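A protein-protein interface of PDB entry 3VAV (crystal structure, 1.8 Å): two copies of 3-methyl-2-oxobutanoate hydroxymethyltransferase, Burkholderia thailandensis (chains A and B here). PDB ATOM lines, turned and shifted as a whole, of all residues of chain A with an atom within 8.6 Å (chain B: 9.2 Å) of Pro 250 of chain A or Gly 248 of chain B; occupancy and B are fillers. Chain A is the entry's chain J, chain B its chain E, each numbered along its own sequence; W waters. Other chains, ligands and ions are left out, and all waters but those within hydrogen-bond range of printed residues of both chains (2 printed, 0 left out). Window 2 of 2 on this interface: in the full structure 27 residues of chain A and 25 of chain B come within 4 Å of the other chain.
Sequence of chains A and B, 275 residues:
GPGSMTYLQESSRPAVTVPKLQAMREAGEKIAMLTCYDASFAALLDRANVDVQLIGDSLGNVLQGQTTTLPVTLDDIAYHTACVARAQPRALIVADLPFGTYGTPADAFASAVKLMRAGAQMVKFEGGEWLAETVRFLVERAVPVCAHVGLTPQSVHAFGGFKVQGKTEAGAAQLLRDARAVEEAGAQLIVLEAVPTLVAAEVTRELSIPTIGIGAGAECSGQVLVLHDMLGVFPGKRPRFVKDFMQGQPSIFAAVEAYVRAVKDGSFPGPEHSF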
ATOM      1  N   PHE A 245       2.938  17.604  30.197  1.00  0.00           N
ATOM      2  CA  PHE A 245       2.259  18.390  31.232  1.00  0.00           C
ATOM      3  C   PHE A 245       0.745  18.404  31.078  1.00  0.00           C
ATOM      4  O   PHE A 245       0.023  18.881  31.954  1.00  0.00           O
ATOM      5  CB  PHE A 245       2.796  19.824  31.261  1.00  0.00           C
ATOM      6  CG  PHE A 245       4.107  19.949  31.986  1.00  0.00           C
ATOM      7  CD1 PHE A 245       4.132  20.176  33.359  1.00  0.00           C
ATOM      8  CD2 PHE A 245       5.301  19.804  31.315  1.00  0.00           C
ATOM      9  CE1 PHE A 245       5.340  20.243  34.048  1.00  0.00           C
ATOM     10  CE2 PHE A 245       6.515  19.889  31.979  1.00  0.00           C
ATOM     11  CZ  PHE A 245       6.537  20.106  33.365  1.00  0.00           C
ATOM     12  N   MET A 246       0.263  17.879  29.965  1.00  0.00           N
ATOM     13  CA  MET A 246      -1.181  17.791  29.732  1.00  0.00           C
ATOM     14  C   MET A 246      -1.837  16.728  30.627  1.00  0.00           C
ATOM     15  O   MET A 246      -2.939  16.937  31.169  1.00  0.00           O
ATOM     16  CB  MET A 246      -1.438  17.504  28.256  1.00  0.00           C
ATOM     17  CG  MET A 246      -2.869  17.647  27.824  1.00  0.00           C
ATOM     18  SD  MET A 246      -3.543  19.314  28.041  1.00  0.00           S
ATOM     19  CE  MET A 246      -4.913  18.907  29.092  1.00  0.00           C
ATOM     20  N   GLN A 247      -1.164  15.601  30.817  1.00  0.00           N
ATOM     21  CA  GLN A 247      -1.761  14.495  31.613  1.00  0.00           C
ATOM     22  C   GLN A 247      -2.150  14.937  33.035  1.00  0.00           C
ATOM     23  O   GLN A 247      -1.363  15.523  33.764  1.00  0.00           O
ATOM     24  CB  GLN A 247      -0.848  13.248  31.613  1.00  0.00           C
ATOM     25  CG  GLN A 247       0.529  13.480  32.145  1.00  0.00           C
ATOM     26  CD  GLN A 247       1.483  12.324  31.868  1.00  0.00           C
ATOM     27  OE1 GLN A 247       2.655  12.546  31.520  1.00  0.00           O
ATOM     28  NE2 GLN A 247       1.002  11.090  32.043  1.00  0.00           N
ATOM     29  N   GLY A 248      -3.413  14.696  33.414  1.00  0.00           N
ATOM     30  CA  GLY A 248      -3.904  15.085  34.734  1.00  0.00           C
ATOM     31  C   GLY A 248      -4.419  16.516  34.834  1.00  0.00           C
ATOM     32  O   GLY A 248      -4.931  16.922  35.875  1.00  0.00           O
ATOM     33  N   GLN A 249      -4.279  17.296  33.769  1.00  0.00           N
ATOM     34  CA  GLN A 249      -4.697  18.700  33.801  1.00  0.00           C
ATOM     35  C   GLN A 249      -6.054  18.857  33.114  1.00  0.00           C
ATOM     36  O   GLN A 249      -6.365  18.129  32.168  1.00  0.00           O
ATOM     37  CB  GLN A 249      -3.655  19.584  33.121  1.00  0.00           C
ATOM     38  CG  GLN A 249      -2.313  19.608  33.845  1.00  0.00           C
ATOM     39  CD  GLN A 249      -2.421  20.199  35.236  1.00  0.00           C
ATOM     40  OE1 GLN A 249      -3.238  21.090  35.483  1.00  0.00           O
ATOM     41  NE2 GLN A 249      -1.646  19.664  36.166  1.00  0.00           N
ATOM     42  N   PRO A 250      -6.850  19.817  33.577  1.00  0.00           N
ATOM     43  CA  PRO A 250      -8.209  19.932  33.066  1.00  0.00           C
ATOM     44  C   PRO A 250      -8.317  20.690  31.733  1.00  0.00           C
ATOM     45  O   PRO A 250      -9.354  20.615  31.073  1.00  0.00           O
ATOM     46  CB  PRO A 250      -8.936  20.686  34.189  1.00  0.00           C
ATOM     47  CG  PRO A 250      -7.867  21.541  34.807  1.00  0.00           C
ATOM     48  CD  PRO A 250      -6.615  20.697  34.742  1.00  0.00           C
ATOM     49  N   SER A 251      -7.245  21.382  31.337  1.00  0.00           N
ATOM     50  CA  SER A 251      -7.253  22.196  30.134  1.00  0.00           C
ATOM     51  C   SER A 251      -5.842  22.405  29.593  1.00  0.00           C
ATOM     52  O   SER A 251      -4.866  22.245  30.314  1.00  0.00           O
ATOM     53  CB  SER A 251      -7.894  23.557  30.399  1.00  0.00           C
ATOM     54  OG  SER A 251      -7.069  24.371  31.230  1.00  0.00           O
ATOM     55  N   ILE A 252      -5.759  22.839  28.334  1.00  0.00           N
ATOM     56  CA  ILE A 252      -4.462  23.140  27.721  1.00  0.00           C
ATOM     57  C   ILE A 252      -3.811  24.318  28.441  1.00  0.00           C
ATOM     58  O   ILE A 252      -2.637  24.281  28.742  1.00  0.00           O
ATOM     59  CB  ILE A 252      -4.596  23.384  26.192  1.00  0.00           C
ATOM     60  CG1 ILE A 252      -5.090  22.086  25.511  1.00  0.00           C
ATOM     61  CG2 ILE A 252      -3.259  23.867  25.605  1.00  0.00           C
ATOM     62  CD1 ILE A 252      -5.441  22.229  24.033  1.00  0.00           C
ATOM     63  N   PHE A 253      -4.594  25.345  28.762  1.00  0.00           N
ATOM     64  CA  PHE A 253      -4.106  26.426  29.613  1.00  0.00           C
ATOM     65  C   PHE A 253      -3.479  25.927  30.913  1.00  0.00           C
ATOM     66  O   PHE A 253      -2.375  26.332  31.256  1.00  0.00           O
ATOM     67  CB  PHE A 253      -5.221  27.415  29.937  1.00  0.00           C
ATOM     68  CG  PHE A 253      -4.806  28.478  30.906  1.00  0.00           C
ATOM     69  CD1 PHE A 253      -3.903  29.452  30.536  1.00  0.00           C
ATOM     70  CD2 PHE A 253      -5.297  28.480  32.202  1.00  0.00           C
ATOM     71  CE1 PHE A 253      -3.503  30.419  31.441  1.00  0.00           C
ATOM     72  CE2 PHE A 253      -4.914  29.453  33.105  1.00  0.00           C
ATOM     73  CZ  PHE A 253      -4.011  30.423  32.721  1.00  0.00           C
ATOM     74  N   ALA A 254      -4.180  25.048  31.628  1.00  0.00           N
ATOM     75  CA  ALA A 254      -3.662  24.511  32.890  1.00  0.00           C
ATOM     76  C   ALA A 254      -2.365  23.732  32.694  1.00  0.00           C
ATOM     77  O   ALA A 254      -1.486  23.732  33.587  1.00  0.00           O
ATOM     78  CB  ALA A 254      -4.705  23.635  33.563  1.00  0.00           C
ATOM     79  N   ALA A 255      -2.246  23.033  31.565  1.00  0.00           N
ATOM     80  CA  ALA A 255      -1.015  22.295  31.262  1.00  0.00           C
ATOM     81  C   ALA A 255       0.169  23.267  31.141  1.00  0.00           C
ATOM     82  O   ALA A 255       1.255  23.038  31.706  1.00  0.00           O
ATOM     83  CB  ALA A 255      -1.171  21.480  29.984  1.00  0.00           C
ATOM     84  N   GLU A 257       0.337  26.348  32.362  1.00  0.00           N
ATOM     85  CA  GLU A 257       0.623  26.920  33.704  1.00  0.00           C
ATOM     86  C   GLU A 257       1.454  25.954  34.529  1.00  0.00           C
ATOM     87  O   GLU A 257       2.301  26.380  35.300  1.00  0.00           O
ATOM     88  CB  GLU A 257      -0.625  27.203  34.532  1.00  0.00           C
ATOM     89  CG  GLU A 257      -1.604  28.206  34.024  1.00  0.00           C
ATOM     90  CD  GLU A 257      -2.740  28.335  35.030  1.00  0.00           C
ATOM     91  OE1 GLU A 257      -3.539  27.365  35.149  1.00  0.00           O
ATOM     92  OE2 GLU A 257      -2.778  29.347  35.758  1.00  0.00           O
ATOM     93  N   ALA A 258       1.168  24.658  34.406  1.00  0.00           N
ATOM     94  CA  ALA A 258       1.868  23.624  35.191  1.00  0.00           C
ATOM     95  C   ALA A 258       3.341  23.566  34.809  1.00  0.00           C
ATOM     96  O   ALA A 258       4.204  23.459  35.676  1.00  0.00           O
ATOM     97  CB  ALA A 258       1.217  22.258  35.019  1.00  0.00           C
ATOM     98  N   ARG A 261       5.015  26.748  36.246  1.00  0.00           N
ATOM     99  CA  ARG A 261       5.153  26.561  37.710  1.00  0.00           C
ATOM    100  C   ARG A 261       6.297  25.593  38.052  1.00  0.00           C
ATOM    101  O   ARG A 261       7.095  25.865  38.959  1.00  0.00           O
ATOM    102  CB  ARG A 261       3.827  26.062  38.285  1.00  0.00           C
ATOM    103  CG  ARG A 261       3.853  25.763  39.791  1.00  0.00           C
ATOM    104  CD  ARG A 261       2.456  25.727  40.402  1.00  0.00           C
ATOM    105  NE  ARG A 261       1.476  25.031  39.549  1.00  0.00           N
ATOM    106  CZ  ARG A 261       0.490  25.619  38.842  1.00  0.00           C
ATOM    107  NH1 ARG A 261      -0.305  24.863  38.087  1.00  0.00           N
ATOM    108  NH2 ARG A 261       0.285  26.947  38.887  1.00  0.00           N
ATOM    109  N   LEU B 231     -10.925  22.296  21.215  1.00  0.00           N
ATOM    110  CA  LEU B 231      -9.916  22.066  22.258  1.00  0.00           C
ATOM    111  C   LEU B 231      -9.885  23.162  23.324  1.00  0.00           C
ATOM    112  O   LEU B 231      -9.033  23.141  24.206  1.00  0.00           O
ATOM    113  CB  LEU B 231      -8.522  21.933  21.644  1.00  0.00           C
ATOM    114  CG  LEU B 231      -8.321  20.728  20.716  1.00  0.00           C
ATOM    115  CD1 LEU B 231      -6.923  20.766  20.154  1.00  0.00           C
ATOM    116  CD2 LEU B 231      -8.588  19.402  21.421  1.00  0.00           C
ATOM    117  N   GLY B 232     -10.809  24.120  23.218  1.00  0.00           N
ATOM    118  CA  GLY B 232     -10.986  25.163  24.217  1.00  0.00           C
ATOM    119  C   GLY B 232      -9.860  26.165  24.304  1.00  0.00           C
ATOM    120  O   GLY B 232      -9.659  26.785  25.352  1.00  0.00           O
ATOM    121  N   LYS B 243     -18.695  23.211  21.201  1.00  0.00           N
ATOM    122  CA  LYS B 243     -18.444  22.643  22.507  1.00  0.00           C
ATOM    123  C   LYS B 243     -16.938  22.460  22.693  1.00  0.00           C
ATOM    124  O   LYS B 243     -16.215  22.104  21.760  1.00  0.00           O
ATOM    125  CB  LYS B 243     -19.148  21.304  22.676  1.00  0.00           C
ATOM    126  CG  LYS B 243     -18.722  20.551  23.930  1.00  0.00           C
ATOM    127  CD  LYS B 243     -19.557  19.303  24.133  1.00  0.00           C
ATOM    128  CE  LYS B 243     -19.090  18.524  25.336  1.00  0.00           C
ATOM    129  NZ  LYS B 243     -19.983  17.368  25.608  1.00  0.00           N
ATOM    130  N   ASP B 244     -16.495  22.707  23.914  1.00  0.00           N
ATOM    131  CA  ASP B 244     -15.127  22.478  24.332  1.00  0.00           C
ATOM    132  C   ASP B 244     -15.059  21.026  24.759  1.00  0.00           C
ATOM    133  O   ASP B 244     -15.508  20.666  25.857  1.00  0.00           O
ATOM    134  CB  ASP B 244     -14.800  23.428  25.484  1.00  0.00           C
ATOM    135  CG  ASP B 244     -13.408  23.210  26.084  1.00  0.00           C
ATOM    136  OD1 ASP B 244     -12.731  22.233  25.726  1.00  0.00           O
ATOM    137  OD2 ASP B 244     -13.013  24.050  26.918  1.00  0.00           O
ATOM    138  N   PHE B 245     -14.488  20.189  23.901  1.00  0.00           N
ATOM    139  CA  PHE B 245     -14.406  18.761  24.164  1.00  0.00           C
ATOM    140  C   PHE B 245     -13.171  18.405  24.992  1.00  0.00           C
ATOM    141  O   PHE B 245     -13.025  17.279  25.430  1.00  0.00           O
ATOM    142  CB  PHE B 245     -14.426  17.970  22.852  1.00  0.00           C
ATOM    143  CG  PHE B 245     -15.806  17.679  22.338  1.00  0.00           C
ATOM    144  CD1 PHE B 245     -16.488  16.532  22.749  1.00  0.00           C
ATOM    145  CD2 PHE B 245     -16.437  18.541  21.458  1.00  0.00           C
ATOM    146  CE1 PHE B 245     -17.768  16.262  22.283  1.00  0.00           C
ATOM    147  CE2 PHE B 245     -17.699  18.265  20.974  1.00  0.00           C
ATOM    148  CZ  PHE B 245     -18.375  17.125  21.395  1.00  0.00           C
ATOM    149  N   MET B 246     -12.304  19.377  25.221  1.00  0.00           N
ATOM    150  CA  MET B 246     -11.102  19.164  26.020  1.00  0.00           C
ATOM    151  C   MET B 246     -11.399  19.187  27.522  1.00  0.00           C
ATOM    152  O   MET B 246     -10.902  18.351  28.260  1.00  0.00           O
ATOM    153  CB  MET B 246     -10.044  20.217  25.663  1.00  0.00           C
ATOM    154  CG  MET B 246      -8.719  20.029  26.353  1.00  0.00           C
ATOM    155  SD  MET B 246      -7.927  18.505  25.839  1.00  0.00           S
ATOM    156  CE  MET B 246      -7.543  17.778  27.422  1.00  0.00           C
ATOM    157  N   GLN B 247     -12.238  20.129  27.965  1.00  0.00           N
ATOM    158  CA  GLN B 247     -12.468  20.332  29.397  1.00  0.00           C
ATOM    159  C   GLN B 247     -12.868  19.007  30.072  1.00  0.00           C
ATOM    160  O   GLN B 247     -13.816  18.338  29.656  1.00  0.00           O
ATOM    161  CB  GLN B 247     -13.527  21.429  29.636  1.00  0.00           C
ATOM    162  CG  GLN B 247     -13.585  21.972  31.078  1.00  0.00           C
ATOM    163  CD  GLN B 247     -12.311  22.711  31.520  1.00  0.00           C
ATOM    164  OE1 GLN B 247     -11.696  23.443  30.742  1.00  0.00           O
ATOM    165  NE2 GLN B 247     -11.933  22.538  32.791  1.00  0.00           N
ATOM    166  N   GLY B 248     -12.088  18.594  31.064  1.00  0.00           N
ATOM    167  CA  GLY B 248     -12.366  17.362  31.797  1.00  0.00           C
ATOM    168  C   GLY B 248     -11.790  16.066  31.215  1.00  0.00           C
ATOM    169  O   GLY B 248     -11.820  15.033  31.879  1.00  0.00           O
ATOM    170  N   GLN B 249     -11.266  16.095  29.989  1.00  0.00           N
ATOM    171  CA  GLN B 249     -10.672  14.878  29.388  1.00  0.00           C
ATOM    172  C   GLN B 249      -9.216  14.681  29.827  1.00  0.00           C
ATOM    173  O   GLN B 249      -8.533  15.642  30.166  1.00  0.00           O
ATOM    174  CB  GLN B 249     -10.772  14.928  27.851  1.00  0.00           C
ATOM    175  CG  GLN B 249     -12.211  14.911  27.342  1.00  0.00           C
ATOM    176  CD  GLN B 249     -12.874  13.562  27.482  1.00  0.00           C
ATOM    177  OE1 GLN B 249     -12.208  12.545  27.665  1.00  0.00           O
ATOM    178  NE2 GLN B 249     -14.201  13.545  27.397  1.00  0.00           N
ATOM    179  N   PRO B 250      -8.729  13.426  29.811  1.00  0.00           N
ATOM    180  CA  PRO B 250      -7.388  13.150  30.311  1.00  0.00           C
ATOM    181  C   PRO B 250      -6.244  13.484  29.327  1.00  0.00           C
ATOM    182  O   PRO B 250      -5.076  13.522  29.743  1.00  0.00           O
ATOM    183  CB  PRO B 250      -7.440  11.649  30.576  1.00  0.00           C
ATOM    184  CG  PRO B 250      -8.374  11.134  29.531  1.00  0.00           C
ATOM    185  CD  PRO B 250      -9.404  12.198  29.350  1.00  0.00           C
ATOM    186  N   SER B 251      -6.577  13.710  28.051  1.00  0.00           N
ATOM    187  CA  SER B 251      -5.577  14.000  27.011  1.00  0.00           C
ATOM    188  C   SER B 251      -6.231  14.694  25.804  1.00  0.00           C
ATOM    189  O   SER B 251      -7.456  14.628  25.604  1.00  0.00           O
ATOM    190  CB  SER B 251      -4.893  12.713  26.545  1.00  0.00           C
ATOM    191  OG  SER B 251      -5.805  11.873  25.847  1.00  0.00           O
ATOM    192  N   ILE B 252      -5.411  15.349  24.989  1.00  0.00           N
ATOM    193  CA  ILE B 252      -5.898  15.916  23.742  1.00  0.00           C
ATOM    194  C   ILE B 252      -6.476  14.834  22.828  1.00  0.00           C
ATOM    195  O   ILE B 252      -7.522  15.027  22.193  1.00  0.00           O
ATOM    196  CB  ILE B 252      -4.796  16.731  23.038  1.00  0.00           C
ATOM    197  CG1 ILE B 252      -4.475  17.969  23.897  1.00  0.00           C
ATOM    198  CG2 ILE B 252      -5.239  17.145  21.622  1.00  0.00           C
ATOM    199  CD1 ILE B 252      -3.259  18.767  23.446  1.00  0.00           C
ATOM    200  N   ALA B 254      -7.995  12.170  23.777  1.00  0.00           N
ATOM    201  CA  ALA B 254      -9.304  11.753  24.319  1.00  0.00           C
ATOM    202  C   ALA B 254     -10.374  12.767  23.992  1.00  0.00           C
ATOM    203  O   ALA B 254     -11.530  12.397  23.760  1.00  0.00           O
ATOM    204  CB  ALA B 254      -9.238  11.517  25.835  1.00  0.00           C
ATOM    205  N   ALA B 255      -9.980  14.044  23.904  1.00  0.00           N
ATOM    206  CA  ALA B 255     -10.892  15.112  23.524  1.00  0.00           C
ATOM    207  C   ALA B 255     -11.376  14.947  22.081  1.00  0.00           C
ATOM    208  O   ALA B 255     -12.551  15.089  21.803  1.00  0.00           O
ATOM    209  CB  ALA B 255     -10.232  16.476  23.712  1.00  0.00           C
ATOM    210  N   ALA B 258     -13.633  12.038  21.870  1.00  0.00           N
ATOM    211  CA  ALA B 258     -14.948  12.341  22.458  1.00  0.00           C
ATOM    212  C   ALA B 258     -15.810  13.091  21.457  1.00  0.00           C
ATOM    213  O   ALA B 258     -17.008  12.840  21.378  1.00  0.00           O
ATOM    214  CB  ALA B 258     -14.823  13.118  23.757  1.00  0.00           C
HETATM  215  O   HOH W   1      -8.293  23.426  26.812  1.00  0.00           O
HETATM  216  O   HOH W   2      -7.171  26.026  27.657  1.00  0.00           O
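Pro 250 of chain A touches just these residues of chain B: Met 246, Gln 247 and Gly 248.
Gly 248 of chain B touches just one residue of chain A: Pro 250.
Printed residues of chain A within 4 Å of Gln 247 of chain B: Pro 250 (3.5 Å) and Ser 251 (3.8 Å).
Printed residues of chain A within 4 Å of Leu 231 of chain B: Ile 252.
Of the printed residues of chain A, Met 246 of chain B touches Met 246 and Pro 250.
Of the printed residues of chain B, Gln 247 of chain A touches Pro 250.
Of the printed residues of chain B, Ile 252 of chain A touches Leu 231.
Ala 255 of chain A touches none of the printed residues of chain B.
Ala 254 of chain A touches none of the printed residues of chain B.
Water W1 lies within hydrogen-bond range of the backbone carbonyl oxygen (O) of Leu 231 of chain B (2.7 Å) and the backbone NH (N) of Ile 252 of chain A (3.0 Å).
Water W2 bridges the backbone NH of Phe 253 of chain A and the backbone carbonyl oxygen of Gly 232 of chain B.
Of the 15 printed residues of chain B, 6 touch a printed residue of chain A.
Hydrophobic or aromatic side chains of chain B that line the printed part of chain A: Leu 231 and Met 246.
Along chain B the printed residues that touch a printed residue of chain A span positions 231 to 250.
Of the 14 printed residues of chain A, 6 touch a printed residue of chain B.
Among the printed residues, no Asp or Glu carboxylate lies within 4 Å of a Lys or Arg side-chain nitrogen of the other chain.
CE of Met 246 of chain A touches CE of Met 246 of chain B, at 3.3 Å.
Gln 247 of chain A touches Pro 250 of chain B (CA to O, 3.9 Å).
O of Gln 249 of chain B touches O of Gln 249 of chain A, 3.9 Å away.
Pro 250 of chain A touches Met 246 of chain B (O to O, 3.9 Å).
Pro 250 of chain A touches Gln 247 of chain B (O to CA, 3.5 Å).
Ser 251 of chain A touches Gln 247 of chain B (CB to OE1, 3.8 Å).
Ile 252 of chain A touches Leu 231 of chain B.
Gln 247 of chain A touches Pro 250 of chain B, and with the chains exchanged Pro 250 of chain A touches Gln 247 of chain B.
Gln 249 of chain A touches its own counterpart, Gln 249 of chain B.
Pro 250 of chain A touches Met 246 of chain B, but with the chains exchanged Met 246 of chain A does not touch Pro 250 of chain B (4.3 Å).
Pro 250 of chain A touches Gly 248 of chain B, but with the chains exchanged Gly 248 of chain A does not touch Pro 250 of chain B (4.2 Å).
The side-chain carboxylate (OD1) of Asp 244 of chain B is in hydrogen-bond range of the backbone NH (N) of Gln 247 of chain B, 3.1 Å away.
N of Ala 254 of chain A lies within hydrogen-bond range of OG of Ser 251 of chain A, 3.0 Å away.
The side-chain carboxylate (OD1) of Asp 244 of chain B is in hydrogen-bond range of the backbone NH (N) of Met 246 of chain B.
N of Gly 248 of chain B sits at hydrogen-bond distance from O of Pro 250 of chain A, at 3.4 Å.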
